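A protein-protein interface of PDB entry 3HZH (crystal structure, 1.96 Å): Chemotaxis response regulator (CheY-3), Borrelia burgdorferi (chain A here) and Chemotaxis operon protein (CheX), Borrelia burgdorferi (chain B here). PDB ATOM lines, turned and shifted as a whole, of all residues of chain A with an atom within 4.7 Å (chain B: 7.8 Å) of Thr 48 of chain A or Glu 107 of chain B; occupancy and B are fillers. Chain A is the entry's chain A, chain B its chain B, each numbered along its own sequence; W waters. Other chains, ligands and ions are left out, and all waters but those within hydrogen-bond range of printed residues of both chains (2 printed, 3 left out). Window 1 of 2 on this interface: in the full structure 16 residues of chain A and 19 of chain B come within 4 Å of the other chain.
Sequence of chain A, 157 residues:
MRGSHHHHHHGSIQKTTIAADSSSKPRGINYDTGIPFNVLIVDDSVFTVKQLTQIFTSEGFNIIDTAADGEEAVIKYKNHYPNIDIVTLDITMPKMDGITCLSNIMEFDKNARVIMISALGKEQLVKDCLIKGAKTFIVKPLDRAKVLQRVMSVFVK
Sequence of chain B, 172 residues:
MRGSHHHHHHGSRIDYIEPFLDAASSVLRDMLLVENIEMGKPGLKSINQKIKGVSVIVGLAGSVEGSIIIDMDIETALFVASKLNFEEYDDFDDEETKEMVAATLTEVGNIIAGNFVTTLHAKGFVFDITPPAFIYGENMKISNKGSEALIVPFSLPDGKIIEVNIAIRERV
Among the printed residues, pairs that only touch across the chains: Ser 45 of chain A with Glu 107 of chain B (3.7 Å), Val 46 of chain A with Met 100 of chain B (3.8 Å), Val 46 of chain A with Ala 103 of chain B (3.1 Å), Phe 47 of chain A with Leu 84 of chain B (3.5 Å), Phe 47 of chain A with Asn 85 of chain B (3.3 Å), Phe 47 of chain A with Met 100 of chain B (3.7 Å), Phe 47 of chain A with Ala 103 of chain B (3.9 Å), Phe 47 of chain A with Thr 104 of chain B (3.4 Å) and Phe 47 of chain A with Glu 107 of chain B (3.996 Å).
N of Ser 45 of chain A is in hydrogen-bond range of OD1 of Asp 43 of chain A (2.9 Å).
NZ of Lys 140 of chain A lies within salt-bridge range of OD2 of Asp 43 of chain A (2.7 Å).
The side-chain sulfur (SD) of Met 100 of chain B lies close to the side-chain amide oxygen (OD1) of Asn 85 of chain B (3.8 Å).
The side-chain amide nitrogen of Asn 85 of chain B is in hydrogen-bond range of the side-chain hydroxyl of Thr 104 of chain B (3.0 Å).
The backbone carbonyl oxygen of Ala 103 of chain B is in hydrogen-bond range of the side-chain hydroxyl of Thr 106 of chain B (3.2 Å).
The side-chain carboxylate of Glu 107 of chain B sits close to the side-chain amide oxygen of Asn 110 of chain B.
Of the 24 printed residues of chain B, 6 touch a printed residue of chain A.
Hydrophobic or aromatic side chains of chain B that line the printed part of chain A: Met 100 and Ala 103.
Printed residues of chain A that touch a printed residue of chain B: Ser 45, Val 46, Phe 47, Thr 48, Lys 50 and Lys 140.
Of chain B, only Glu 107 (2.4 Å) comes within 4 Å of Thr 48 of chain A.
Of the printed residues of chain A, Glu 107 of chain B touches Ser 45, Phe 47, Thr 48 and Lys 140.
Printed residues of chain B within 4 Å of Lys 140 of chain A: Glu 107.
Of the printed residues of chain B, Ser 45 of chain A touches Ala 103 and Glu 107.
Of the printed residues of chain B, Phe 47 of chain A touches Leu 84 (3.5 Å), Asn 85 (3.3 Å), Met 100 (3.7 Å), Ala 103 (3.9 Å), Thr 104 (3.4 Å) and Glu 107 (3.996 Å).
Of the printed residues of chain B, Lys 50 of chain A touches Asn 85.
Val 27 of chain B touches none of the printed residues of chain A.
The nearest printed residue of chain A that does not touch Leu 84 of chain B is Gln 51 of chain A (5.5 Å).
The backbone carbonyl oxygen of Ala 103 of chain B lies within hydrogen-bond range of the side-chain hydroxyl of Ser 45 of chain A.
The side-chain carboxylate (OE2) of Glu 107 of chain B lies within hydrogen-bond range of the side-chain hydroxyl (OG1) of Thr 48 of chain A (2.4 Å).
The side-chain amide oxygen of Asn 85 of chain B lies within hydrogen-bond range of the side-chain amino group of Lys 50 of chain A.
OE2 of Glu 107 of chain B is in salt-bridge range of NZ of Lys 140 of chain A (2.8 Å).
Water W1 lies within hydrogen-bond range of OG1 of Thr 106 of chain B (2.8 Å), OG of Ser 45 of chain A (3.1 Å) and O of Ala 103 of chain B (3.4 Å).
Water W2 lies within hydrogen-bond range of OE2 of Glu 107 of chain B (2.9 Å) and OG1 of Thr 48 of chain A (3.1 Å).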
ATOM      1  N   ASP A  43      28.372  25.687  10.070  1.00  0.00           N
ATOM      2  CA  ASP A  43      28.914  24.729   9.109  1.00  0.00           C
ATOM      3  C   ASP A  43      30.125  25.380   8.449  1.00  0.00           C
ATOM      4  O   ASP A  43      30.124  26.579   8.202  1.00  0.00           O
ATOM      5  CB  ASP A  43      27.856  24.375   8.055  1.00  0.00           C
ATOM      6  CG  ASP A  43      28.219  23.134   7.266  1.00  0.00           C
ATOM      7  OD1 ASP A  43      29.185  23.178   6.469  1.00  0.00           O
ATOM      8  OD2 ASP A  43      27.534  22.103   7.452  1.00  0.00           O
ATOM      9  N   SER A  45      31.091  25.089   5.475  1.00  0.00           N
ATOM     10  CA  SER A  45      30.880  25.320   4.047  1.00  0.00           C
ATOM     11  C   SER A  45      29.884  26.450   3.794  1.00  0.00           C
ATOM     12  O   SER A  45      28.721  26.354   4.185  1.00  0.00           O
ATOM     13  CB  SER A  45      30.360  24.055   3.356  1.00  0.00           C
ATOM     14  OG  SER A  45      30.125  24.317   1.979  1.00  0.00           O
ATOM     15  N   VAL A  46      30.327  27.508   3.124  1.00  0.00           N
ATOM     16  CA  VAL A  46      29.441  28.628   2.827  1.00  0.00           C
ATOM     17  C   VAL A  46      28.297  28.163   1.927  1.00  0.00           C
ATOM     18  O   VAL A  46      27.239  28.789   1.875  1.00  0.00           O
ATOM     19  CB  VAL A  46      30.188  29.796   2.133  1.00  0.00           C
ATOM     20  CG1 VAL A  46      31.305  30.296   3.028  1.00  0.00           C
ATOM     21  CG2 VAL A  46      30.731  29.352   0.793  1.00  0.00           C
ATOM     22  N   PHE A  47      28.512  27.071   1.209  1.00  0.00           N
ATOM     23  CA  PHE A  47      27.467  26.524   0.351  1.00  0.00           C
ATOM     24  C   PHE A  47      26.319  26.047   1.230  1.00  0.00           C
ATOM     25  O   PHE A  47      25.148  26.380   1.013  1.00  0.00           O
ATOM     26  CB  PHE A  47      27.998  25.338  -0.458  1.00  0.00           C
ATOM     27  CG  PHE A  47      26.913  24.501  -1.109  1.00  0.00           C
ATOM     28  CD1 PHE A  47      26.151  24.994  -2.161  1.00  0.00           C
ATOM     29  CD2 PHE A  47      26.639  23.221  -0.644  1.00  0.00           C
ATOM     30  CE1 PHE A  47      25.132  24.246  -2.748  1.00  0.00           C
ATOM     31  CE2 PHE A  47      25.625  22.456  -1.219  1.00  0.00           C
ATOM     32  CZ  PHE A  47      24.866  22.976  -2.277  1.00  0.00           C
ATOM     33  N   THR A  48      26.673  25.256   2.234  1.00  0.00           N
ATOM     34  CA  THR A  48      25.693  24.701   3.154  1.00  0.00           C
ATOM     35  C   THR A  48      25.051  25.793   4.004  1.00  0.00           C
ATOM     36  O   THR A  48      23.865  25.732   4.301  1.00  0.00           O
ATOM     37  CB  THR A  48      26.348  23.648   4.056  1.00  0.00           C
ATOM     38  OG1 THR A  48      26.970  22.653   3.230  1.00  0.00           O
ATOM     39  CG2 THR A  48      25.313  22.971   4.933  1.00  0.00           C
ATOM     40  N   VAL A  49      25.836  26.787   4.395  1.00  0.00           N
ATOM     41  CA  VAL A  49      25.295  27.882   5.188  1.00  0.00           C
ATOM     42  C   VAL A  49      24.209  28.567   4.350  1.00  0.00           C
ATOM     43  O   VAL A  49      23.136  28.896   4.856  1.00  0.00           O
ATOM     44  CB  VAL A  49      26.409  28.885   5.578  1.00  0.00           C
ATOM     45  CG1 VAL A  49      25.805  30.125   6.244  1.00  0.00           C
ATOM     46  CG2 VAL A  49      27.394  28.206   6.530  1.00  0.00           C
ATOM     47  N   LYS A  50      24.479  28.750   3.061  1.00  0.00           N
ATOM     48  CA  LYS A  50      23.502  29.383   2.181  1.00  0.00           C
ATOM     49  C   LYS A  50      22.240  28.529   1.991  1.00  0.00           C
ATOM     50  O   LYS A  50      21.126  29.058   1.970  1.00  0.00           O
ATOM     51  CB  LYS A  50      24.118  29.686   0.813  1.00  0.00           C
ATOM     52  CG  LYS A  50      23.170  30.472  -0.087  1.00  0.00           C
ATOM     53  CD  LYS A  50      23.793  30.883  -1.413  1.00  0.00           C
ATOM     54  CE  LYS A  50      23.989  29.696  -2.340  1.00  0.00           C
ATOM     55  NZ  LYS A  50      24.500  30.147  -3.663  1.00  0.00           N
ATOM     56  N   GLN A  51      22.403  27.212   1.872  1.00  0.00           N
ATOM     57  CA  GLN A  51      21.254  26.334   1.665  1.00  0.00           C
ATOM     58  C   GLN A  51      20.330  26.396   2.884  1.00  0.00           C
ATOM     59  O   GLN A  51      19.121  26.578   2.754  1.00  0.00           O
ATOM     60  CB  GLN A  51      21.734  24.899   1.424  1.00  0.00           C
ATOM     61  CG  GLN A  51      20.898  24.086   0.429  1.00  0.00           C
ATOM     62  CD  GLN A  51      21.440  22.666   0.253  1.00  0.00           C
ATOM     63  OE1 GLN A  51      22.401  22.283   0.909  1.00  0.00           O
ATOM     64  NE2 GLN A  51      20.813  21.895  -0.619  1.00  0.00           N
ATOM     65  N   LEU A  52      20.916  26.242   4.066  1.00  0.00           N
ATOM     66  CA  LEU A  52      20.184  26.301   5.322  1.00  0.00           C
ATOM     67  C   LEU A  52      19.544  27.690   5.493  1.00  0.00           C
ATOM     68  O   LEU A  52      18.408  27.813   5.958  1.00  0.00           O
ATOM     69  CB  LEU A  52      21.148  25.985   6.481  1.00  0.00           C
ATOM     70  CG  LEU A  52      21.153  24.594   7.159  1.00  0.00           C
ATOM     71  CD1 LEU A  52      20.530  23.529   6.288  1.00  0.00           C
ATOM     72  CD2 LEU A  52      22.585  24.231   7.551  1.00  0.00           C
ATOM     73  N   LYS A 140      23.088  14.448   5.826  1.00  0.00           N
ATOM     74  CA  LYS A 140      23.144  15.076   4.505  1.00  0.00           C
ATOM     75  C   LYS A 140      23.170  13.971   3.434  1.00  0.00           C
ATOM     76  O   LYS A 140      23.540  12.830   3.735  1.00  0.00           O
ATOM     77  CB  LYS A 140      24.390  15.955   4.406  1.00  0.00           C
ATOM     78  CG  LYS A 140      24.507  17.033   5.490  1.00  0.00           C
ATOM     79  CD  LYS A 140      25.823  17.796   5.362  1.00  0.00           C
ATOM     80  CE  LYS A 140      25.906  18.987   6.325  1.00  0.00           C
ATOM     81  NZ  LYS A 140      27.206  19.728   6.154  1.00  0.00           N
ATOM     82  N   LEU A 142      20.916  17.390   2.063  1.00  0.00           N
ATOM     83  CA  LEU A 142      19.719  18.104   2.489  1.00  0.00           C
ATOM     84  C   LEU A 142      18.608  18.369   1.476  1.00  0.00           C
ATOM     85  O   LEU A 142      18.840  18.468   0.274  1.00  0.00           O
ATOM     86  CB  LEU A 142      20.139  19.460   3.053  1.00  0.00           C
ATOM     87  CG  LEU A 142      21.200  19.361   4.140  1.00  0.00           C
ATOM     88  CD1 LEU A 142      21.649  20.739   4.573  1.00  0.00           C
ATOM     89  CD2 LEU A 142      20.625  18.575   5.296  1.00  0.00           C
ATOM     90  N   VAL B  27      25.658   9.663  -3.778  1.00  0.00           N
ATOM     91  CA  VAL B  27      25.681  11.086  -3.447  1.00  0.00           C
ATOM     92  C   VAL B  27      25.594  12.005  -4.666  1.00  0.00           C
ATOM     93  O   VAL B  27      24.848  12.988  -4.650  1.00  0.00           O
ATOM     94  CB  VAL B  27      26.942  11.467  -2.637  1.00  0.00           C
ATOM     95  CG1 VAL B  27      26.960  12.970  -2.381  1.00  0.00           C
ATOM     96  CG2 VAL B  27      26.955  10.728  -1.315  1.00  0.00           C
ATOM     97  N   MET B  31      22.654  14.685  -5.241  1.00  0.00           N
ATOM     98  CA  MET B  31      22.940  16.119  -5.195  1.00  0.00           C
ATOM     99  C   MET B  31      22.728  16.808  -6.549  1.00  0.00           C
ATOM    100  O   MET B  31      21.893  17.705  -6.666  1.00  0.00           O
ATOM    101  CB  MET B  31      24.372  16.375  -4.695  1.00  0.00           C
ATOM    102  CG  MET B  31      24.698  15.735  -3.340  1.00  0.00           C
ATOM    103  SD  MET B  31      26.177  16.402  -2.484  1.00  0.00           S
ATOM    104  CE  MET B  31      25.543  18.054  -2.020  1.00  0.00           C
ATOM    105  N   VAL B  56      39.398  18.122  -4.921  1.00  0.00           N
ATOM    106  CA  VAL B  56      38.925  18.176  -3.555  1.00  0.00           C
ATOM    107  C   VAL B  56      39.585  16.999  -2.856  1.00  0.00           C
ATOM    108  O   VAL B  56      39.634  15.897  -3.399  1.00  0.00           O
ATOM    109  CB  VAL B  56      37.397  18.041  -3.490  1.00  0.00           C
ATOM    110  CG1 VAL B  56      36.946  17.913  -2.056  1.00  0.00           C
ATOM    111  CG2 VAL B  56      36.752  19.258  -4.145  1.00  0.00           C
ATOM    112  N   VAL B  58      39.769  14.818   0.804  1.00  0.00           N
ATOM    113  CA  VAL B  58      39.249  14.522   2.122  1.00  0.00           C
ATOM    114  C   VAL B  58      40.093  13.373   2.664  1.00  0.00           C
ATOM    115  O   VAL B  58      40.120  12.278   2.100  1.00  0.00           O
ATOM    116  CB  VAL B  58      37.772  14.122   2.077  1.00  0.00           C
ATOM    117  CG1 VAL B  58      37.277  13.798   3.495  1.00  0.00           C
ATOM    118  CG2 VAL B  58      36.951  15.261   1.483  1.00  0.00           C
ATOM    119  N   ILE B  70      38.561  14.099  -5.412  1.00  0.00           N
ATOM    120  CA  ILE B  70      37.643  14.319  -6.525  1.00  0.00           C
ATOM    121  C   ILE B  70      38.262  15.344  -7.461  1.00  0.00           C
ATOM    122  O   ILE B  70      38.615  16.444  -7.034  1.00  0.00           O
ATOM    123  CB  ILE B  70      36.296  14.852  -6.030  1.00  0.00           C
ATOM    124  CG1 ILE B  70      35.666  13.840  -5.076  1.00  0.00           C
ATOM    125  CG2 ILE B  70      35.384  15.135  -7.213  1.00  0.00           C
ATOM    126  CD1 ILE B  70      34.372  14.308  -4.464  1.00  0.00           C
ATOM    127  N   LEU B  84      24.235  22.848  -8.512  1.00  0.00           N
ATOM    128  CA  LEU B  84      23.977  22.730  -7.080  1.00  0.00           C
ATOM    129  C   LEU B  84      23.478  23.996  -6.375  1.00  0.00           C
ATOM    130  O   LEU B  84      22.798  23.930  -5.345  1.00  0.00           O
ATOM    131  CB  LEU B  84      25.192  22.173  -6.342  1.00  0.00           C
ATOM    132  CG  LEU B  84      25.653  20.800  -6.842  1.00  0.00           C
ATOM    133  CD1 LEU B  84      26.657  20.209  -5.866  1.00  0.00           C
ATOM    134  CD2 LEU B  84      24.464  19.874  -6.975  1.00  0.00           C
ATOM    135  N   ASN B  85      23.803  25.147  -6.934  1.00  0.00           N
ATOM    136  CA  ASN B  85      23.381  26.409  -6.361  1.00  0.00           C
ATOM    137  C   ASN B  85      22.199  26.986  -7.138  1.00  0.00           C
ATOM    138  O   ASN B  85      21.689  28.067  -6.808  1.00  0.00           O
ATOM    139  CB  ASN B  85      24.561  27.376  -6.388  1.00  0.00           C
ATOM    140  CG  ASN B  85      25.563  27.094  -5.310  1.00  0.00           C
ATOM    141  OD1 ASN B  85      25.382  27.511  -4.161  1.00  0.00           O
ATOM    142  ND2 ASN B  85      26.618  26.362  -5.656  1.00  0.00           N
ATOM    143  N   MET B 100      32.360  30.324  -3.891  1.00  0.00           N
ATOM    144  CA  MET B 100      31.254  29.387  -3.815  1.00  0.00           C
ATOM    145  C   MET B 100      31.575  28.086  -4.543  1.00  0.00           C
ATOM    146  O   MET B 100      31.144  27.027  -4.105  1.00  0.00           O
ATOM    147  CB  MET B 100      29.965  30.011  -4.365  1.00  0.00           C
ATOM    148  CG  MET B 100      28.708  29.175  -4.092  1.00  0.00           C
ATOM    149  SD  MET B 100      28.360  28.931  -2.308  1.00  0.00           S
ATOM    150  CE  MET B 100      28.208  30.649  -1.768  1.00  0.00           C
ATOM    151  N   VAL B 101      32.330  28.159  -5.643  1.00  0.00           N
ATOM    152  CA  VAL B 101      32.705  26.949  -6.384  1.00  0.00           C
ATOM    153  C   VAL B 101      33.475  26.008  -5.457  1.00  0.00           C
ATOM    154  O   VAL B 101      33.136  24.827  -5.325  1.00  0.00           O
ATOM    155  CB  VAL B 101      33.591  27.274  -7.621  1.00  0.00           C
ATOM    156  CG1 VAL B 101      34.234  26.001  -8.160  1.00  0.00           C
ATOM    157  CG2 VAL B 101      32.741  27.896  -8.719  1.00  0.00           C
ATOM    158  N   ALA B 102      34.507  26.549  -4.812  1.00  0.00           N
ATOM    159  CA  ALA B 102      35.331  25.786  -3.884  1.00  0.00           C
ATOM    160  C   ALA B 102      34.497  25.196  -2.752  1.00  0.00           C
ATOM    161  O   ALA B 102      34.555  23.996  -2.486  1.00  0.00           O
ATOM    162  CB  ALA B 102      36.429  26.674  -3.298  1.00  0.00           C
ATOM    163  N   ALA B 103      33.713  26.045  -2.097  1.00  0.00           N
ATOM    164  CA  ALA B 103      32.874  25.618  -0.974  1.00  0.00           C
ATOM    165  C   ALA B 103      31.850  24.554  -1.342  1.00  0.00           C
ATOM    166  O   ALA B 103      31.514  23.694  -0.521  1.00  0.00           O
ATOM    167  CB  ALA B 103      32.167  26.821  -0.371  1.00  0.00           C
ATOM    168  N   THR B 104      31.340  24.624  -2.570  1.00  0.00           N
ATOM    169  CA  THR B 104      30.356  23.661  -3.031  1.00  0.00           C
ATOM    170  C   THR B 104      30.996  22.312  -3.337  1.00  0.00           C
ATOM    171  O   THR B 104      30.515  21.275  -2.887  1.00  0.00           O
ATOM    172  CB  THR B 104      29.619  24.157  -4.304  1.00  0.00           C
ATOM    173  OG1 THR B 104      28.997  25.427  -4.048  1.00  0.00           O
ATOM    174  CG2 THR B 104      28.535  23.155  -4.709  1.00  0.00           C
ATOM    175  N   LEU B 105      32.077  22.313  -4.107  1.00  0.00           N
ATOM    176  CA  LEU B 105      32.739  21.052  -4.445  1.00  0.00           C
ATOM    177  C   LEU B 105      33.347  20.350  -3.228  1.00  0.00           C
ATOM    178  O   LEU B 105      33.288  19.116  -3.128  1.00  0.00           O
ATOM    179  CB  LEU B 105      33.813  21.281  -5.512  1.00  0.00           C
ATOM    180  CG  LEU B 105      33.313  21.904  -6.818  1.00  0.00           C
ATOM    181  CD1 LEU B 105      34.452  21.941  -7.831  1.00  0.00           C
ATOM    182  CD2 LEU B 105      32.141  21.100  -7.357  1.00  0.00           C
ATOM    183  N   THR B 106      33.929  21.113  -2.301  1.00  0.00           N
ATOM    184  CA  THR B 106      34.499  20.488  -1.107  1.00  0.00           C
ATOM    185  C   THR B 106      33.380  19.867  -0.275  1.00  0.00           C
ATOM    186  O   THR B 106      33.582  18.835   0.357  1.00  0.00           O
ATOM    187  CB  THR B 106      35.298  21.489  -0.216  1.00  0.00           C
ATOM    188  OG1 THR B 106      34.461  22.595   0.161  1.00  0.00           O
ATOM    189  CG2 THR B 106      36.534  21.996  -0.953  1.00  0.00           C
ATOM    190  N   GLU B 107      32.197  20.479  -0.282  1.00  0.00           N
ATOM    191  CA  GLU B 107      31.077  19.931   0.483  1.00  0.00           C
ATOM    192  C   GLU B 107      30.602  18.637  -0.173  1.00  0.00           C
ATOM    193  O   GLU B 107      30.147  17.717   0.513  1.00  0.00           O
ATOM    194  CB  GLU B 107      29.908  20.930   0.574  1.00  0.00           C
ATOM    195  CG  GLU B 107      28.678  20.366   1.270  1.00  0.00           C
ATOM    196  CD  GLU B 107      28.818  20.252   2.779  1.00  0.00           C
ATOM    197  OE1 GLU B 107      29.941  20.000   3.262  1.00  0.00           O
ATOM    198  OE2 GLU B 107      27.794  20.385   3.488  1.00  0.00           O
ATOM    199  N   VAL B 108      30.693  18.563  -1.500  1.00  0.00           N
ATOM    200  CA  VAL B 108      30.307  17.335  -2.191  1.00  0.00           C
ATOM    201  C   VAL B 108      31.274  16.244  -1.716  1.00  0.00           C
ATOM    202  O   VAL B 108      30.862  15.119  -1.431  1.00  0.00           O
ATOM    203  CB  VAL B 108      30.423  17.460  -3.738  1.00  0.00           C
ATOM    204  CG1 VAL B 108      30.261  16.085  -4.383  1.00  0.00           C
ATOM    205  CG2 VAL B 108      29.334  18.412  -4.286  1.00  0.00           C
ATOM    206  N   GLY B 109      32.555  16.591  -1.629  1.00  0.00           N
ATOM    207  CA  GLY B 109      33.569  15.642  -1.187  1.00  0.00           C
ATOM    208  C   GLY B 109      33.293  15.176   0.232  1.00  0.00           C
ATOM    209  O   GLY B 109      33.352  13.981   0.537  1.00  0.00           O
ATOM    210  N   ASN B 110      32.990  16.140   1.094  1.00  0.00           N
ATOM    211  CA  ASN B 110      32.671  15.879   2.488  1.00  0.00           C
ATOM    212  C   ASN B 110      31.485  14.916   2.625  1.00  0.00           C
ATOM    213  O   ASN B 110      31.485  14.015   3.481  1.00  0.00           O
ATOM    214  CB  ASN B 110      32.340  17.200   3.191  1.00  0.00           C
ATOM    215  CG  ASN B 110      31.854  16.990   4.609  1.00  0.00           C
ATOM    216  OD1 ASN B 110      30.820  17.549   5.001  1.00  0.00           O
ATOM    217  ND2 ASN B 110      32.588  16.216   5.388  1.00  0.00           N
ATOM    218  N   ILE B 111      30.477  15.096   1.781  1.00  0.00           N
ATOM    219  CA  ILE B 111      29.300  14.241   1.862  1.00  0.00           C
ATOM    220  C   ILE B 111      29.582  12.835   1.347  1.00  0.00           C
ATOM    221  O   ILE B 111      29.118  11.858   1.938  1.00  0.00           O
ATOM    222  CB  ILE B 111      28.105  14.905   1.136  1.00  0.00           C
ATOM    223  CG1 ILE B 111      27.817  16.255   1.818  1.00  0.00           C
ATOM    224  CG2 ILE B 111      26.862  14.004   1.204  1.00  0.00           C
ATOM    225  CD1 ILE B 111      26.794  17.129   1.105  1.00  0.00           C
ATOM    226  N   ILE B 112      30.346  12.722   0.260  1.00  0.00           N
ATOM    227  CA  ILE B 112      30.693  11.404  -0.267  1.00  0.00           C
ATOM    228  C   ILE B 112      31.505  10.674   0.809  1.00  0.00           C
ATOM    229  O   ILE B 112      31.170   9.560   1.200  1.00  0.00           O
ATOM    230  CB  ILE B 112      31.551  11.501  -1.551  1.00  0.00           C
ATOM    231  CG1 ILE B 112      30.706  12.066  -2.704  1.00  0.00           C
ATOM    232  CG2 ILE B 112      32.124  10.134  -1.897  1.00  0.00           C
ATOM    233  CD1 ILE B 112      31.489  12.303  -4.009  1.00  0.00           C
ATOM    234  N   ALA B 113      32.551  11.330   1.302  1.00  0.00           N
ATOM    235  CA  ALA B 113      33.415  10.749   2.327  1.00  0.00           C
ATOM    236  C   ALA B 113      32.683  10.379   3.614  1.00  0.00           C
ATOM    237  O   ALA B 113      32.952   9.331   4.199  1.00  0.00           O
ATOM    238  CB  ALA B 113      34.559  11.699   2.651  1.00  0.00           C
ATOM    239  N   GLY B 114      31.768  11.240   4.051  1.00  0.00           N
ATOM    240  CA  GLY B 114      31.023  10.976   5.266  1.00  0.00           C
ATOM    241  C   GLY B 114      30.097   9.785   5.114  1.00  0.00           C
ATOM    242  O   GLY B 114      30.054   8.904   5.979  1.00  0.00           O
ATOM    243  N   PRO B 132      37.727  19.202   4.458  1.00  0.00           N
ATOM    244  CA  PRO B 132      38.236  19.135   3.090  1.00  0.00           C
ATOM    245  C   PRO B 132      39.210  20.210   2.649  1.00  0.00           C
ATOM    246  O   PRO B 132      39.300  21.285   3.242  1.00  0.00           O
ATOM    247  CB  PRO B 132      36.950  19.168   2.274  1.00  0.00           C
ATOM    248  CG  PRO B 132      36.177  20.228   3.036  1.00  0.00           C
ATOM    249  CD  PRO B 132      36.352  19.735   4.472  1.00  0.00           C
ATOM    250  N   PHE B 134      40.669  22.294  -0.939  1.00  0.00           N
ATOM    251  CA  PHE B 134      40.350  22.609  -2.319  1.00  0.00           C
ATOM    252  C   PHE B 134      41.657  22.984  -2.995  1.00  0.00           C
ATOM    253  O   PHE B 134      42.341  23.912  -2.563  1.00  0.00           O
ATOM    254  CB  PHE B 134      39.367  23.785  -2.410  1.00  0.00           C
ATOM    255  CG  PHE B 134      38.877  24.061  -3.811  1.00  0.00           C
ATOM    256  CD1 PHE B 134      38.085  23.133  -4.479  1.00  0.00           C
ATOM    257  CD2 PHE B 134      39.218  25.241  -4.465  1.00  0.00           C
ATOM    258  CE1 PHE B 134      37.631  23.373  -5.779  1.00  0.00           C
ATOM    259  CE2 PHE B 134      38.771  25.492  -5.768  1.00  0.00           C
ATOM    260  CZ  PHE B 134      37.976  24.555  -6.426  1.00  0.00           C
HETATM  261  O   HOH W   1      32.952  23.111   2.463  1.00  0.00           O
HETATM  262  O   HOH W   2      25.048  20.342   2.547  1.00  0.00           O
